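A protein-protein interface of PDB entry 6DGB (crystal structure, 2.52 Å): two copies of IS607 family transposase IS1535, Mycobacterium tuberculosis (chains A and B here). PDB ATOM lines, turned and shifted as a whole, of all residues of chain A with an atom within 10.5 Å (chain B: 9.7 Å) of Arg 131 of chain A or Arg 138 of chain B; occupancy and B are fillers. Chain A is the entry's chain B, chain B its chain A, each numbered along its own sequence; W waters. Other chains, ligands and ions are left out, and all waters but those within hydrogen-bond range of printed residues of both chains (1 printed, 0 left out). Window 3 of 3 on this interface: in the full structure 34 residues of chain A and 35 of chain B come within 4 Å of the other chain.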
ATOM      1  N   VAL A 105       5.871  -6.602   9.863  1.00  0.00           N
ATOM      2  CA  VAL A 105       4.451  -6.886  10.107  1.00  0.00           C
ATOM      3  C   VAL A 105       4.081  -8.265   9.546  1.00  0.00           C
ATOM      4  O   VAL A 105       3.382  -9.046  10.206  1.00  0.00           O
ATOM      5  CB  VAL A 105       3.551  -5.732   9.596  1.00  0.00           C
ATOM      6  CG1 VAL A 105       3.937  -5.281   8.179  1.00  0.00           C
ATOM      7  CG2 VAL A 105       2.071  -6.066   9.704  1.00  0.00           C
ATOM      8  N   MET A 108       5.677 -10.672  11.860  1.00  0.00           N
ATOM      9  CA  MET A 108       4.943 -10.690  13.136  1.00  0.00           C
ATOM     10  C   MET A 108       3.828 -11.739  13.026  1.00  0.00           C
ATOM     11  O   MET A 108       3.579 -12.457  13.992  1.00  0.00           O
ATOM     12  CB  MET A 108       4.338  -9.294  13.400  1.00  0.00           C
ATOM     13  CG  MET A 108       4.281  -8.893  14.869  1.00  0.00           C
ATOM     14  SD  MET A 108       4.332  -7.100  15.203  1.00  0.00           S
ATOM     15  CE  MET A 108       2.694  -6.574  14.644  1.00  0.00           C
ATOM     16  N   ILE A 109       3.180 -11.839  11.836  1.00  0.00           N
ATOM     17  CA  ILE A 109       2.124 -12.811  11.550  1.00  0.00           C
ATOM     18  C   ILE A 109       2.720 -14.219  11.473  1.00  0.00           C
ATOM     19  O   ILE A 109       2.194 -15.121  12.120  1.00  0.00           O
ATOM     20  CB  ILE A 109       1.287 -12.443  10.295  1.00  0.00           C
ATOM     21  CG1 ILE A 109       0.636 -11.079  10.462  1.00  0.00           C
ATOM     22  CG2 ILE A 109       0.210 -13.485  10.015  1.00  0.00           C
ATOM     23  CD1 ILE A 109       0.201 -10.424   9.174  1.00  0.00           C
ATOM     24  N   LEU A 112       3.665 -15.349  15.112  1.00  0.00           N
ATOM     25  CA  LEU A 112       2.467 -15.578  15.906  1.00  0.00           C
ATOM     26  C   LEU A 112       1.681 -16.787  15.416  1.00  0.00           C
ATOM     27  O   LEU A 112       1.167 -17.512  16.259  1.00  0.00           O
ATOM     28  CB  LEU A 112       1.580 -14.342  15.946  1.00  0.00           C
ATOM     29  CG  LEU A 112       1.911 -13.295  16.998  1.00  0.00           C
ATOM     30  CD1 LEU A 112       1.458 -11.926  16.537  1.00  0.00           C
ATOM     31  CD2 LEU A 112       1.236 -13.615  18.331  1.00  0.00           C
ATOM     32  N   THR A 113       1.633 -17.048  14.085  1.00  0.00           N
ATOM     33  CA  THR A 113       0.951 -18.229  13.547  1.00  0.00           C
ATOM     34  C   THR A 113       1.573 -19.503  14.140  1.00  0.00           C
ATOM     35  O   THR A 113       0.857 -20.266  14.785  1.00  0.00           O
ATOM     36  CB  THR A 113       0.904 -18.234  11.998  1.00  0.00           C
ATOM     37  OG1 THR A 113       0.156 -17.103  11.550  1.00  0.00           O
ATOM     38  CG2 THR A 113       0.239 -19.472  11.437  1.00  0.00           C
ATOM     39  N   CYS A 116       1.131 -19.821  17.852  1.00  0.00           N
ATOM     40  CA  CYS A 116      -0.300 -20.125  18.105  1.00  0.00           C
ATOM     41  C   CYS A 116      -0.586 -21.596  17.782  1.00  0.00           C
ATOM     42  O   CYS A 116      -1.395 -22.216  18.467  1.00  0.00           O
ATOM     43  CB  CYS A 116      -1.223 -19.218  17.288  1.00  0.00           C
ATOM     44  SG  CYS A 116      -1.479 -17.570  17.988  1.00  0.00           S
ATOM     45  N   LEU A 119       0.741 -23.678  20.553  1.00  0.00           N
ATOM     46  CA  LEU A 119      -0.057 -23.433  21.749  1.00  0.00           C
ATOM     47  C   LEU A 119      -1.490 -23.949  21.725  1.00  0.00           C
ATOM     48  O   LEU A 119      -1.913 -24.573  22.694  1.00  0.00           O
ATOM     49  CB  LEU A 119      -0.071 -21.932  22.062  1.00  0.00           C
ATOM     50  CG  LEU A 119       1.070 -21.410  22.912  1.00  0.00           C
ATOM     51  CD1 LEU A 119       1.307 -19.950  22.666  1.00  0.00           C
ATOM     52  CD2 LEU A 119       0.814 -21.645  24.369  1.00  0.00           C
ATOM     53  N   TYR A 120      -2.272 -23.638  20.675  1.00  0.00           N
ATOM     54  CA  TYR A 120      -3.698 -23.989  20.669  1.00  0.00           C
ATOM     55  C   TYR A 120      -4.157 -24.834  19.502  1.00  0.00           C
ATOM     56  O   TYR A 120      -5.365 -25.039  19.344  1.00  0.00           O
ATOM     57  CB  TYR A 120      -4.558 -22.714  20.767  1.00  0.00           C
ATOM     58  CG  TYR A 120      -3.903 -21.587  21.540  1.00  0.00           C
ATOM     59  CD1 TYR A 120      -3.864 -21.601  22.929  1.00  0.00           C
ATOM     60  CD2 TYR A 120      -3.295 -20.523  20.878  1.00  0.00           C
ATOM     61  CE1 TYR A 120      -3.232 -20.586  23.644  1.00  0.00           C
ATOM     62  CE2 TYR A 120      -2.681 -19.490  21.582  1.00  0.00           C
ATOM     63  CZ  TYR A 120      -2.649 -19.527  22.968  1.00  0.00           C
ATOM     64  OH  TYR A 120      -2.044 -18.523  23.684  1.00  0.00           O
ATOM     65  N   GLY A 121      -3.211 -25.352  18.724  1.00  0.00           N
ATOM     66  CA  GLY A 121      -3.494 -26.165  17.545  1.00  0.00           C
ATOM     67  C   GLY A 121      -3.443 -25.357  16.265  1.00  0.00           C
ATOM     68  O   GLY A 121      -3.789 -24.171  16.270  1.00  0.00           O
ATOM     69  N   ARG A 123      -5.364 -25.388  13.643  1.00  0.00           N
ATOM     70  CA  ARG A 123      -6.690 -24.989  13.157  1.00  0.00           C
ATOM     71  C   ARG A 123      -6.971 -23.547  13.567  1.00  0.00           C
ATOM     72  O   ARG A 123      -7.036 -23.250  14.763  1.00  0.00           O
ATOM     73  CB  ARG A 123      -7.781 -25.961  13.666  1.00  0.00           C
ATOM     74  CG  ARG A 123      -8.999 -26.069  12.743  1.00  0.00           C
ATOM     75  N   GLY A 124      -7.009 -22.663  12.570  1.00  0.00           N
ATOM     76  CA  GLY A 124      -7.229 -21.233  12.752  1.00  0.00           C
ATOM     77  C   GLY A 124      -6.079 -20.439  13.359  1.00  0.00           C
ATOM     78  O   GLY A 124      -6.261 -19.266  13.689  1.00  0.00           O
ATOM     79  N   ALA A 125      -4.874 -21.043  13.487  1.00  0.00           N
ATOM     80  CA  ALA A 125      -3.690 -20.399  14.070  1.00  0.00           C
ATOM     81  C   ALA A 125      -3.296 -19.066  13.414  1.00  0.00           C
ATOM     82  O   ALA A 125      -2.820 -18.165  14.099  1.00  0.00           O
ATOM     83  CB  ALA A 125      -2.512 -21.369  14.077  1.00  0.00           C
ATOM     84  N   ARG A 126      -3.515 -18.929  12.091  1.00  0.00           N
ATOM     85  CA  ARG A 126      -3.227 -17.698  11.357  1.00  0.00           C
ATOM     86  C   ARG A 126      -4.306 -16.634  11.639  1.00  0.00           C
ATOM     87  O   ARG A 126      -3.982 -15.453  11.749  1.00  0.00           O
ATOM     88  CB  ARG A 126      -3.055 -17.963   9.863  1.00  0.00           C
ATOM     89  CG  ARG A 126      -2.491 -16.752   9.150  1.00  0.00           C
ATOM     90  CD  ARG A 126      -1.846 -17.027   7.825  1.00  0.00           C
ATOM     91  NE  ARG A 126      -2.098 -15.887   6.954  1.00  0.00           N
ATOM     92  CZ  ARG A 126      -1.230 -14.918   6.683  1.00  0.00           C
ATOM     93  NH1 ARG A 126      -1.590 -13.892   5.924  1.00  0.00           N
ATOM     94  NH2 ARG A 126       0.014 -14.985   7.137  1.00  0.00           N
ATOM     95  N   ASN A 127      -5.570 -17.053  11.797  1.00  0.00           N
ATOM     96  CA  ASN A 127      -6.654 -16.138  12.138  1.00  0.00           C
ATOM     97  C   ASN A 127      -6.436 -15.516  13.540  1.00  0.00           C
ATOM     98  O   ASN A 127      -6.683 -14.324  13.710  1.00  0.00           O
ATOM     99  CB  ASN A 127      -8.002 -16.836  12.011  1.00  0.00           C
ATOM    100  CG  ASN A 127      -8.378 -17.185  10.585  1.00  0.00           C
ATOM    101  OD1 ASN A 127      -8.028 -16.491   9.616  1.00  0.00           O
ATOM    102  ND2 ASN A 127      -9.122 -18.267  10.422  1.00  0.00           N
ATOM    103  N   ARG A 128      -5.891 -16.304  14.503  1.00  0.00           N
ATOM    104  CA  ARG A 128      -5.496 -15.880  15.862  1.00  0.00           C
ATOM    105  C   ARG A 128      -4.370 -14.827  15.748  1.00  0.00           C
ATOM    106  O   ARG A 128      -4.530 -13.704  16.222  1.00  0.00           O
ATOM    107  CB  ARG A 128      -4.977 -17.081  16.678  1.00  0.00           C
ATOM    108  CG  ARG A 128      -5.997 -18.165  16.989  1.00  0.00           C
ATOM    109  CD  ARG A 128      -5.291 -19.307  17.694  1.00  0.00           C
ATOM    110  NE  ARG A 128      -6.219 -20.371  18.057  1.00  0.00           N
ATOM    111  CZ  ARG A 128      -6.844 -20.451  19.230  1.00  0.00           C
ATOM    112  NH1 ARG A 128      -6.642 -19.530  20.163  1.00  0.00           N
ATOM    113  NH2 ARG A 128      -7.660 -21.465  19.485  1.00  0.00           N
ATOM    114  N   ALA A 129      -3.267 -15.178  15.060  1.00  0.00           N
ATOM    115  CA  ALA A 129      -2.141 -14.297  14.757  1.00  0.00           C
ATOM    116  C   ALA A 129      -2.588 -12.981  14.100  1.00  0.00           C
ATOM    117  O   ALA A 129      -1.986 -11.946  14.375  1.00  0.00           O
ATOM    118  CB  ALA A 129      -1.175 -15.005  13.820  1.00  0.00           C
ATOM    119  N   MET A 130      -3.620 -13.028  13.222  1.00  0.00           N
ATOM    120  CA  MET A 130      -4.160 -11.866  12.497  1.00  0.00           C
ATOM    121  C   MET A 130      -4.869 -10.884  13.414  1.00  0.00           C
ATOM    122  O   MET A 130      -4.702  -9.684  13.239  1.00  0.00           O
ATOM    123  CB  MET A 130      -5.120 -12.290  11.385  1.00  0.00           C
ATOM    124  CG  MET A 130      -4.465 -13.032  10.238  1.00  0.00           C
ATOM    125  SD  MET A 130      -3.178 -12.160   9.326  1.00  0.00           S
ATOM    126  CE  MET A 130      -4.170 -10.889   8.470  1.00  0.00           C
ATOM    127  N   ARG A 131      -5.678 -11.383  14.373  1.00  0.00           N
ATOM    128  CA  ARG A 131      -6.392 -10.550  15.346  1.00  0.00           C
ATOM    129  C   ARG A 131      -5.368  -9.923  16.297  1.00  0.00           C
ATOM    130  O   ARG A 131      -5.580  -8.806  16.774  1.00  0.00           O
ATOM    131  CB  ARG A 131      -7.386 -11.396  16.168  1.00  0.00           C
ATOM    132  CG  ARG A 131      -8.554 -11.962  15.416  1.00  0.00           C
ATOM    133  CD  ARG A 131      -9.360 -12.826  16.337  1.00  0.00           C
ATOM    134  NE  ARG A 131      -9.951 -13.932  15.602  1.00  0.00           N
ATOM    135  CZ  ARG A 131     -10.689 -14.875  16.160  1.00  0.00           C
ATOM    136  NH1 ARG A 131     -10.970 -14.827  17.453  1.00  0.00           N
ATOM    137  NH2 ARG A 131     -11.180 -15.864  15.422  1.00  0.00           N
ATOM    138  N   ALA A 132      -4.282 -10.671  16.589  1.00  0.00           N
ATOM    139  CA  ALA A 132      -3.198 -10.253  17.473  1.00  0.00           C
ATOM    140  C   ALA A 132      -2.389  -9.098  16.881  1.00  0.00           C
ATOM    141  O   ALA A 132      -2.211  -8.086  17.561  1.00  0.00           O
ATOM    142  CB  ALA A 132      -2.286 -11.437  17.791  1.00  0.00           C
ATOM    143  N   VAL A 133      -1.912  -9.255  15.611  1.00  0.00           N
ATOM    144  CA  VAL A 133      -1.133  -8.262  14.838  1.00  0.00           C
ATOM    145  C   VAL A 133      -1.955  -6.973  14.656  1.00  0.00           C
ATOM    146  O   VAL A 133      -1.384  -5.886  14.512  1.00  0.00           O
ATOM    147  CB  VAL A 133      -0.596  -8.857  13.494  1.00  0.00           C
ATOM    148  CG1 VAL A 133      -0.184  -7.775  12.488  1.00  0.00           C
ATOM    149  CG2 VAL A 133       0.569  -9.805  13.750  1.00  0.00           C
ATOM    150  N   THR A 134      -3.293  -7.119  14.719  1.00  0.00           N
ATOM    151  CA  THR A 134      -4.312  -6.082  14.623  1.00  0.00           C
ATOM    152  C   THR A 134      -4.469  -5.329  15.976  1.00  0.00           C
ATOM    153  O   THR A 134      -4.451  -4.091  15.973  1.00  0.00           O
ATOM    154  CB  THR A 134      -5.603  -6.712  14.058  1.00  0.00           C
ATOM    155  OG1 THR A 134      -5.413  -6.959  12.654  1.00  0.00           O
ATOM    156  CG2 THR A 134      -6.858  -5.866  14.300  1.00  0.00           C
ATOM    157  N   GLU A 135      -4.593  -6.053  17.120  1.00  0.00           N
ATOM    158  CA  GLU A 135      -4.732  -5.438  18.458  1.00  0.00           C
ATOM    159  C   GLU A 135      -3.485  -4.622  18.881  1.00  0.00           C
ATOM    160  O   GLU A 135      -3.570  -3.739  19.743  1.00  0.00           O
ATOM    161  CB  GLU A 135      -5.106  -6.485  19.521  1.00  0.00           C
ATOM    162  CG  GLU A 135      -5.730  -5.906  20.789  1.00  0.00           C
ATOM    163  CD  GLU A 135      -7.169  -5.401  20.771  1.00  0.00           C
ATOM    164  OE1 GLU A 135      -7.563  -4.708  19.801  1.00  0.00           O
ATOM    165  OE2 GLU A 135      -7.877  -5.623  21.782  1.00  0.00           O
ATOM    166  N   ALA A 136      -2.340  -4.910  18.245  1.00  0.00           N
ATOM    167  CA  ALA A 136      -1.077  -4.245  18.492  1.00  0.00           C
ATOM    168  C   ALA A 136      -0.855  -3.203  17.392  1.00  0.00           C
ATOM    169  O   ALA A 136       0.128  -3.260  16.649  1.00  0.00           O
ATOM    170  CB  ALA A 136       0.035  -5.276  18.515  1.00  0.00           C
ATOM    171  N   LYS A 137      -1.829  -2.280  17.266  1.00  0.00           N
ATOM    172  CA  LYS A 137      -1.849  -1.164  16.309  1.00  0.00           C
ATOM    173  C   LYS A 137      -2.507   0.116  16.890  1.00  0.00           C
ATOM    174  O   LYS A 137      -2.308   1.195  16.332  1.00  0.00           O
ATOM    175  CB  LYS A 137      -2.520  -1.564  14.984  1.00  0.00           C
ATOM    176  CG  LYS A 137      -1.636  -2.389  14.057  1.00  0.00           C
ATOM    177  CD  LYS A 137      -2.218  -2.452  12.666  1.00  0.00           C
ATOM    178  CE  LYS A 137      -1.635  -3.574  11.850  1.00  0.00           C
ATOM    179  NZ  LYS A 137      -2.295  -3.658  10.522  1.00  0.00           N
ATOM    180  N   ARG A 138      -3.251  -0.005  18.017  1.00  0.00           N
ATOM    181  CA  ARG A 138      -3.949   1.098  18.694  1.00  0.00           C
ATOM    182  C   ARG A 138      -3.080   1.912  19.680  1.00  0.00           C
ATOM    183  O   ARG A 138      -2.979   3.140  19.551  1.00  0.00           O
ATOM    184  CB  ARG A 138      -5.243   0.618  19.386  1.00  0.00           C
ATOM    185  CG  ARG A 138      -5.224  -0.779  20.002  1.00  0.00           C
ATOM    186  CD  ARG A 138      -6.645  -1.301  20.040  1.00  0.00           C
ATOM    187  NE  ARG A 138      -6.957  -2.142  21.198  1.00  0.00           N
ATOM    188  CZ  ARG A 138      -7.283  -1.692  22.409  1.00  0.00           C
ATOM    189  NH1 ARG A 138      -7.558  -2.548  23.391  1.00  0.00           N
ATOM    190  NH2 ARG A 138      -7.285  -0.388  22.664  1.00  0.00           N
ATOM    191  N   MET B 108       6.245 -15.097  23.009  1.00  0.00           N
ATOM    192  CA  MET B 108       5.253 -14.442  22.136  1.00  0.00           C
ATOM    193  C   MET B 108       5.171 -12.950  22.529  1.00  0.00           C
ATOM    194  O   MET B 108       5.073 -12.078  21.664  1.00  0.00           O
ATOM    195  CB  MET B 108       3.883 -15.123  22.306  1.00  0.00           C
ATOM    196  CG  MET B 108       3.040 -15.177  21.050  1.00  0.00           C
ATOM    197  SD  MET B 108       1.892 -16.609  20.980  1.00  0.00           S
ATOM    198  CE  MET B 108       0.593 -16.079  22.113  1.00  0.00           C
ATOM    199  N   LEU B 112       6.521  -9.712  20.224  1.00  0.00           N
ATOM    200  CA  LEU B 112       5.568  -8.655  19.954  1.00  0.00           C
ATOM    201  C   LEU B 112       5.995  -7.329  20.563  1.00  0.00           C
ATOM    202  O   LEU B 112       5.801  -6.315  19.904  1.00  0.00           O
ATOM    203  CB  LEU B 112       4.170  -9.046  20.435  1.00  0.00           C
ATOM    204  CG  LEU B 112       3.314  -9.866  19.486  1.00  0.00           C
ATOM    205  CD1 LEU B 112       2.340 -10.747  20.270  1.00  0.00           C
ATOM    206  CD2 LEU B 112       2.568  -8.950  18.488  1.00  0.00           C
ATOM    207  N   ARG B 128       0.921  -3.132  24.414  1.00  0.00           N
ATOM    208  CA  ARG B 128       0.405  -3.468  23.077  1.00  0.00           C
ATOM    209  C   ARG B 128       0.541  -4.980  22.892  1.00  0.00           C
ATOM    210  O   ARG B 128      -0.459  -5.639  22.639  1.00  0.00           O
ATOM    211  CB  ARG B 128       1.203  -2.756  21.962  1.00  0.00           C
ATOM    212  CG  ARG B 128       1.085  -1.250  21.916  1.00  0.00           C
ATOM    213  CD  ARG B 128       2.026  -0.704  20.860  1.00  0.00           C
ATOM    214  NE  ARG B 128       1.925   0.746  20.740  1.00  0.00           N
ATOM    215  CZ  ARG B 128       1.121   1.370  19.881  1.00  0.00           C
ATOM    216  NH1 ARG B 128       0.347   0.672  19.057  1.00  0.00           N
ATOM    217  NH2 ARG B 128       1.096   2.696  19.827  1.00  0.00           N
ATOM    218  N   ALA B 129       1.768  -5.528  23.056  1.00  0.00           N
ATOM    219  CA  ALA B 129       2.081  -6.956  22.993  1.00  0.00           C
ATOM    220  C   ALA B 129       1.179  -7.793  23.916  1.00  0.00           C
ATOM    221  O   ALA B 129       0.816  -8.909  23.548  1.00  0.00           O
ATOM    222  CB  ALA B 129       3.529  -7.177  23.380  1.00  0.00           C
ATOM    223  N   ARG B 131      -2.045  -7.016  25.059  1.00  0.00           N
ATOM    224  CA  ARG B 131      -3.416  -7.025  24.534  1.00  0.00           C
ATOM    225  C   ARG B 131      -3.474  -7.935  23.298  1.00  0.00           C
ATOM    226  O   ARG B 131      -4.509  -8.549  23.027  1.00  0.00           O
ATOM    227  CB  ARG B 131      -3.865  -5.623  24.116  1.00  0.00           C
ATOM    228  CG  ARG B 131      -3.978  -4.577  25.221  1.00  0.00           C
ATOM    229  CD  ARG B 131      -4.249  -3.166  24.681  1.00  0.00           C
ATOM    230  NE  ARG B 131      -3.569  -2.911  23.402  1.00  0.00           N
ATOM    231  CZ  ARG B 131      -2.996  -1.763  23.039  1.00  0.00           C
ATOM    232  NH1 ARG B 131      -2.962  -0.732  23.879  1.00  0.00           N
ATOM    233  NH2 ARG B 131      -2.421  -1.650  21.845  1.00  0.00           N
ATOM    234  N   ALA B 132      -2.360  -7.996  22.537  1.00  0.00           N
ATOM    235  CA  ALA B 132      -2.208  -8.804  21.327  1.00  0.00           C
ATOM    236  C   ALA B 132      -2.173 -10.288  21.644  1.00  0.00           C
ATOM    237  O   ALA B 132      -2.938 -11.025  21.024  1.00  0.00           O
ATOM    238  CB  ALA B 132      -0.957  -8.403  20.562  1.00  0.00           C
ATOM    239  N   VAL B 133      -1.307 -10.730  22.610  1.00  0.00           N
ATOM    240  CA  VAL B 133      -1.187 -12.127  23.053  1.00  0.00           C
ATOM    241  C   VAL B 133      -2.541 -12.588  23.605  1.00  0.00           C
ATOM    242  O   VAL B 133      -2.922 -13.745  23.437  1.00  0.00           O
ATOM    243  CB  VAL B 133       0.011 -12.319  24.035  1.00  0.00           C
ATOM    244  CG1 VAL B 133      -0.191 -13.483  25.006  1.00  0.00           C
ATOM    245  CG2 VAL B 133       1.309 -12.487  23.259  1.00  0.00           C
ATOM    246  N   THR B 134      -3.297 -11.632  24.163  1.00  0.00           N
ATOM    247  CA  THR B 134      -4.622 -11.821  24.735  1.00  0.00           C
ATOM    248  C   THR B 134      -5.662 -12.067  23.618  1.00  0.00           C
ATOM    249  O   THR B 134      -6.397 -13.042  23.726  1.00  0.00           O
ATOM    250  CB  THR B 134      -4.921 -10.652  25.695  1.00  0.00           C
ATOM    251  OG1 THR B 134      -4.150 -10.837  26.898  1.00  0.00           O
ATOM    252  CG2 THR B 134      -6.411 -10.480  26.008  1.00  0.00           C
ATOM    253  N   GLU B 135      -5.699 -11.227  22.549  1.00  0.00           N
ATOM    254  CA  GLU B 135      -6.643 -11.376  21.420  1.00  0.00           C
ATOM    255  C   GLU B 135      -6.450 -12.687  20.620  1.00  0.00           C
ATOM    256  O   GLU B 135      -7.390 -13.165  19.963  1.00  0.00           O
ATOM    257  CB  GLU B 135      -6.630 -10.147  20.488  1.00  0.00           C
ATOM    258  CG  GLU B 135      -7.895 -10.000  19.632  1.00  0.00           C
ATOM    259  CD  GLU B 135      -9.196  -9.511  20.257  1.00  0.00           C
ATOM    260  OE1 GLU B 135      -9.524  -9.935  21.389  1.00  0.00           O
ATOM    261  OE2 GLU B 135      -9.939  -8.774  19.568  1.00  0.00           O
ATOM    262  N   ALA B 136      -5.245 -13.273  20.722  1.00  0.00           N
ATOM    263  CA  ALA B 136      -4.849 -14.517  20.085  1.00  0.00           C
ATOM    264  C   ALA B 136      -4.962 -15.653  21.094  1.00  0.00           C
ATOM    265  O   ALA B 136      -3.985 -16.360  21.353  1.00  0.00           O
ATOM    266  CB  ALA B 136      -3.422 -14.397  19.576  1.00  0.00           C
ATOM    267  N   LYS B 137      -6.164 -15.802  21.689  1.00  0.00           N
ATOM    268  CA  LYS B 137      -6.501 -16.836  22.675  1.00  0.00           C
ATOM    269  C   LYS B 137      -7.961 -17.327  22.552  1.00  0.00           C
ATOM    270  O   LYS B 137      -8.282 -18.396  23.082  1.00  0.00           O
ATOM    271  CB  LYS B 137      -6.215 -16.354  24.113  1.00  0.00           C
ATOM    272  CG  LYS B 137      -4.751 -16.403  24.530  1.00  0.00           C
ATOM    273  CD  LYS B 137      -4.617 -16.239  26.024  1.00  0.00           C
ATOM    274  CE  LYS B 137      -3.218 -15.845  26.425  1.00  0.00           C
ATOM    275  NZ  LYS B 137      -3.124 -15.636  27.897  1.00  0.00           N
ATOM    276  N   ARG B 138      -8.827 -16.569  21.838  1.00  0.00           N
ATOM    277  CA  ARG B 138     -10.259 -16.863  21.675  1.00  0.00           C
ATOM    278  C   ARG B 138     -10.637 -17.828  20.508  1.00  0.00           C
ATOM    279  O   ARG B 138     -11.217 -18.893  20.776  1.00  0.00           O
ATOM    280  CB  ARG B 138     -11.102 -15.566  21.584  1.00  0.00           C
ATOM    281  CG  ARG B 138     -10.474 -14.385  20.853  1.00  0.00           C
ATOM    282  CD  ARG B 138     -11.092 -13.108  21.363  1.00  0.00           C
ATOM    283  NE  ARG B 138     -11.266 -12.101  20.316  1.00  0.00           N
ATOM    284  CZ  ARG B 138     -12.355 -11.979  19.562  1.00  0.00           C
ATOM    285  NH1 ARG B 138     -13.377 -12.815  19.717  1.00  0.00           N
ATOM    286  NH2 ARG B 138     -12.434 -11.020  18.648  1.00  0.00           N
ATOM    287  N   GLU B 139     -10.390 -17.414  19.232  1.00  0.00           N
ATOM    288  CA  GLU B 139     -10.707 -18.121  17.971  1.00  0.00           C
ATOM    289  C   GLU B 139     -12.218 -18.259  17.735  1.00  0.00           C
ATOM    290  O   GLU B 139     -12.863 -19.174  18.245  1.00  0.00           O
ATOM    291  CB  GLU B 139      -9.981 -19.472  17.830  1.00  0.00           C
HETATM  292  O   HOH W   1      -6.800  -7.389  24.018  1.00  0.00           O
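N of Glu 139 of chain B lies close to NH1 of Arg 131 of chain A, 3.2 Å away.
The guanidinium group (NH2) of Arg 131 of chain B lies within hydrogen-bond range of the backbone carbonyl oxygen (O) of Glu 135 of chain A, 3.2 Å away.
OE1 of Glu 135 of chain B is in salt-bridge range of NE of Arg 138 of chain B (3.0 Å).
The side-chain carboxylate of Glu 135 of chain A is in salt-bridge range of the guanidinium group of Arg 138 of chain A, 3.0 Å away.
The side-chain sulfur of Cys 116 of chain A lies close to the backbone carbonyl oxygen of Leu 112 of chain A, at 3.2 Å.
Among the printed residues, pairs that only touch across the chains: Ala 132 of chain A with Ala 132 of chain B, Tyr 120 of chain A with Ala 136 of chain B, Arg 131 of chain A with Arg 138 of chain B, Arg 138 of chain A with Arg 131 of chain B, Arg 128 of chain A with Glu 139 of chain B, Arg 128 of chain A with Lys 137 of chain B, Tyr 120 of chain A with Lys 137 of chain B, Arg 128 of chain A with Ala 136 of chain B, Leu 112 of chain A with Met 108 of chain B, Lys 137 of chain A with Arg 128 of chain B, Leu 112 of chain A with Leu 112 of chain B, Ala 132 of chain A with Ala 136 of chain B, Arg 138 of chain A with Arg 128 of chain B, Arg 131 of chain A with Glu 135 of chain B, Leu 119 of chain A with Met 108 of chain B, Ala 136 of chain A with Ala 132 of chain B and Tyr 120 of chain A with Met 108 of chain B.
Of the printed residues of chain B, Leu 112 of chain A touches Met 108 (3.6 Å) and Leu 112 (3.6 Å).
Ala 125 of chain A touches none of the printed residues of chain B.
Arg 131 of chain A touches just these residues of chain B: Glu 135, Arg 138 and Glu 139.
No residue of chain B comes within 4 Å of Thr 134 of chain A.
Printed residues of chain A within 4 Å of Leu 112 of chain B: Leu 112 (3.6 Å).
Val 133 of chain B touches none of the printed residues of chain A.
Of chain A, only Arg 131 (3.8 Å) comes within 4 Å of Glu 135 of chain B.
Printed residues of chain A within 4 Å of Ala 136 of chain B: Tyr 120 (3.4 Å), Arg 128 (3.6 Å) and Ala 132 (3.6 Å).
Arg 138 of chain B touches just one residue of chain A: Arg 131.
Glu 139 of chain B touches just these residues of chain A: Arg 128 (3.5 Å) and Arg 131 (3.2 Å).
Leu 112 of chain A touches Met 108 of chain B, but with the chains exchanged Met 108 of chain A does not touch Leu 112 of chain B (4.004 Å).
Arg 131 of chain A touches Glu 135 of chain B, and with the chains exchanged Glu 135 of chain A touches Arg 131 of chain B.
Arg 131 of chain A touches Arg 138 of chain B, and with the chains exchanged Arg 138 of chain A touches Arg 131 of chain B.
Arg 138 of chain A touches Arg 128 of chain B, but with the chains exchanged Arg 128 of chain A does not touch Arg 138 of chain B (4.04 Å).
12 positions are printed for both chains.
Of the 19 pairs that touch across the chains among the printed residues, 10 have their exchanged pair printed and touching as well.
Water W1 bridges O of Arg 131 of chain B (2.8 Å) and OE2 of Glu 135 of chain A (3.0 Å).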
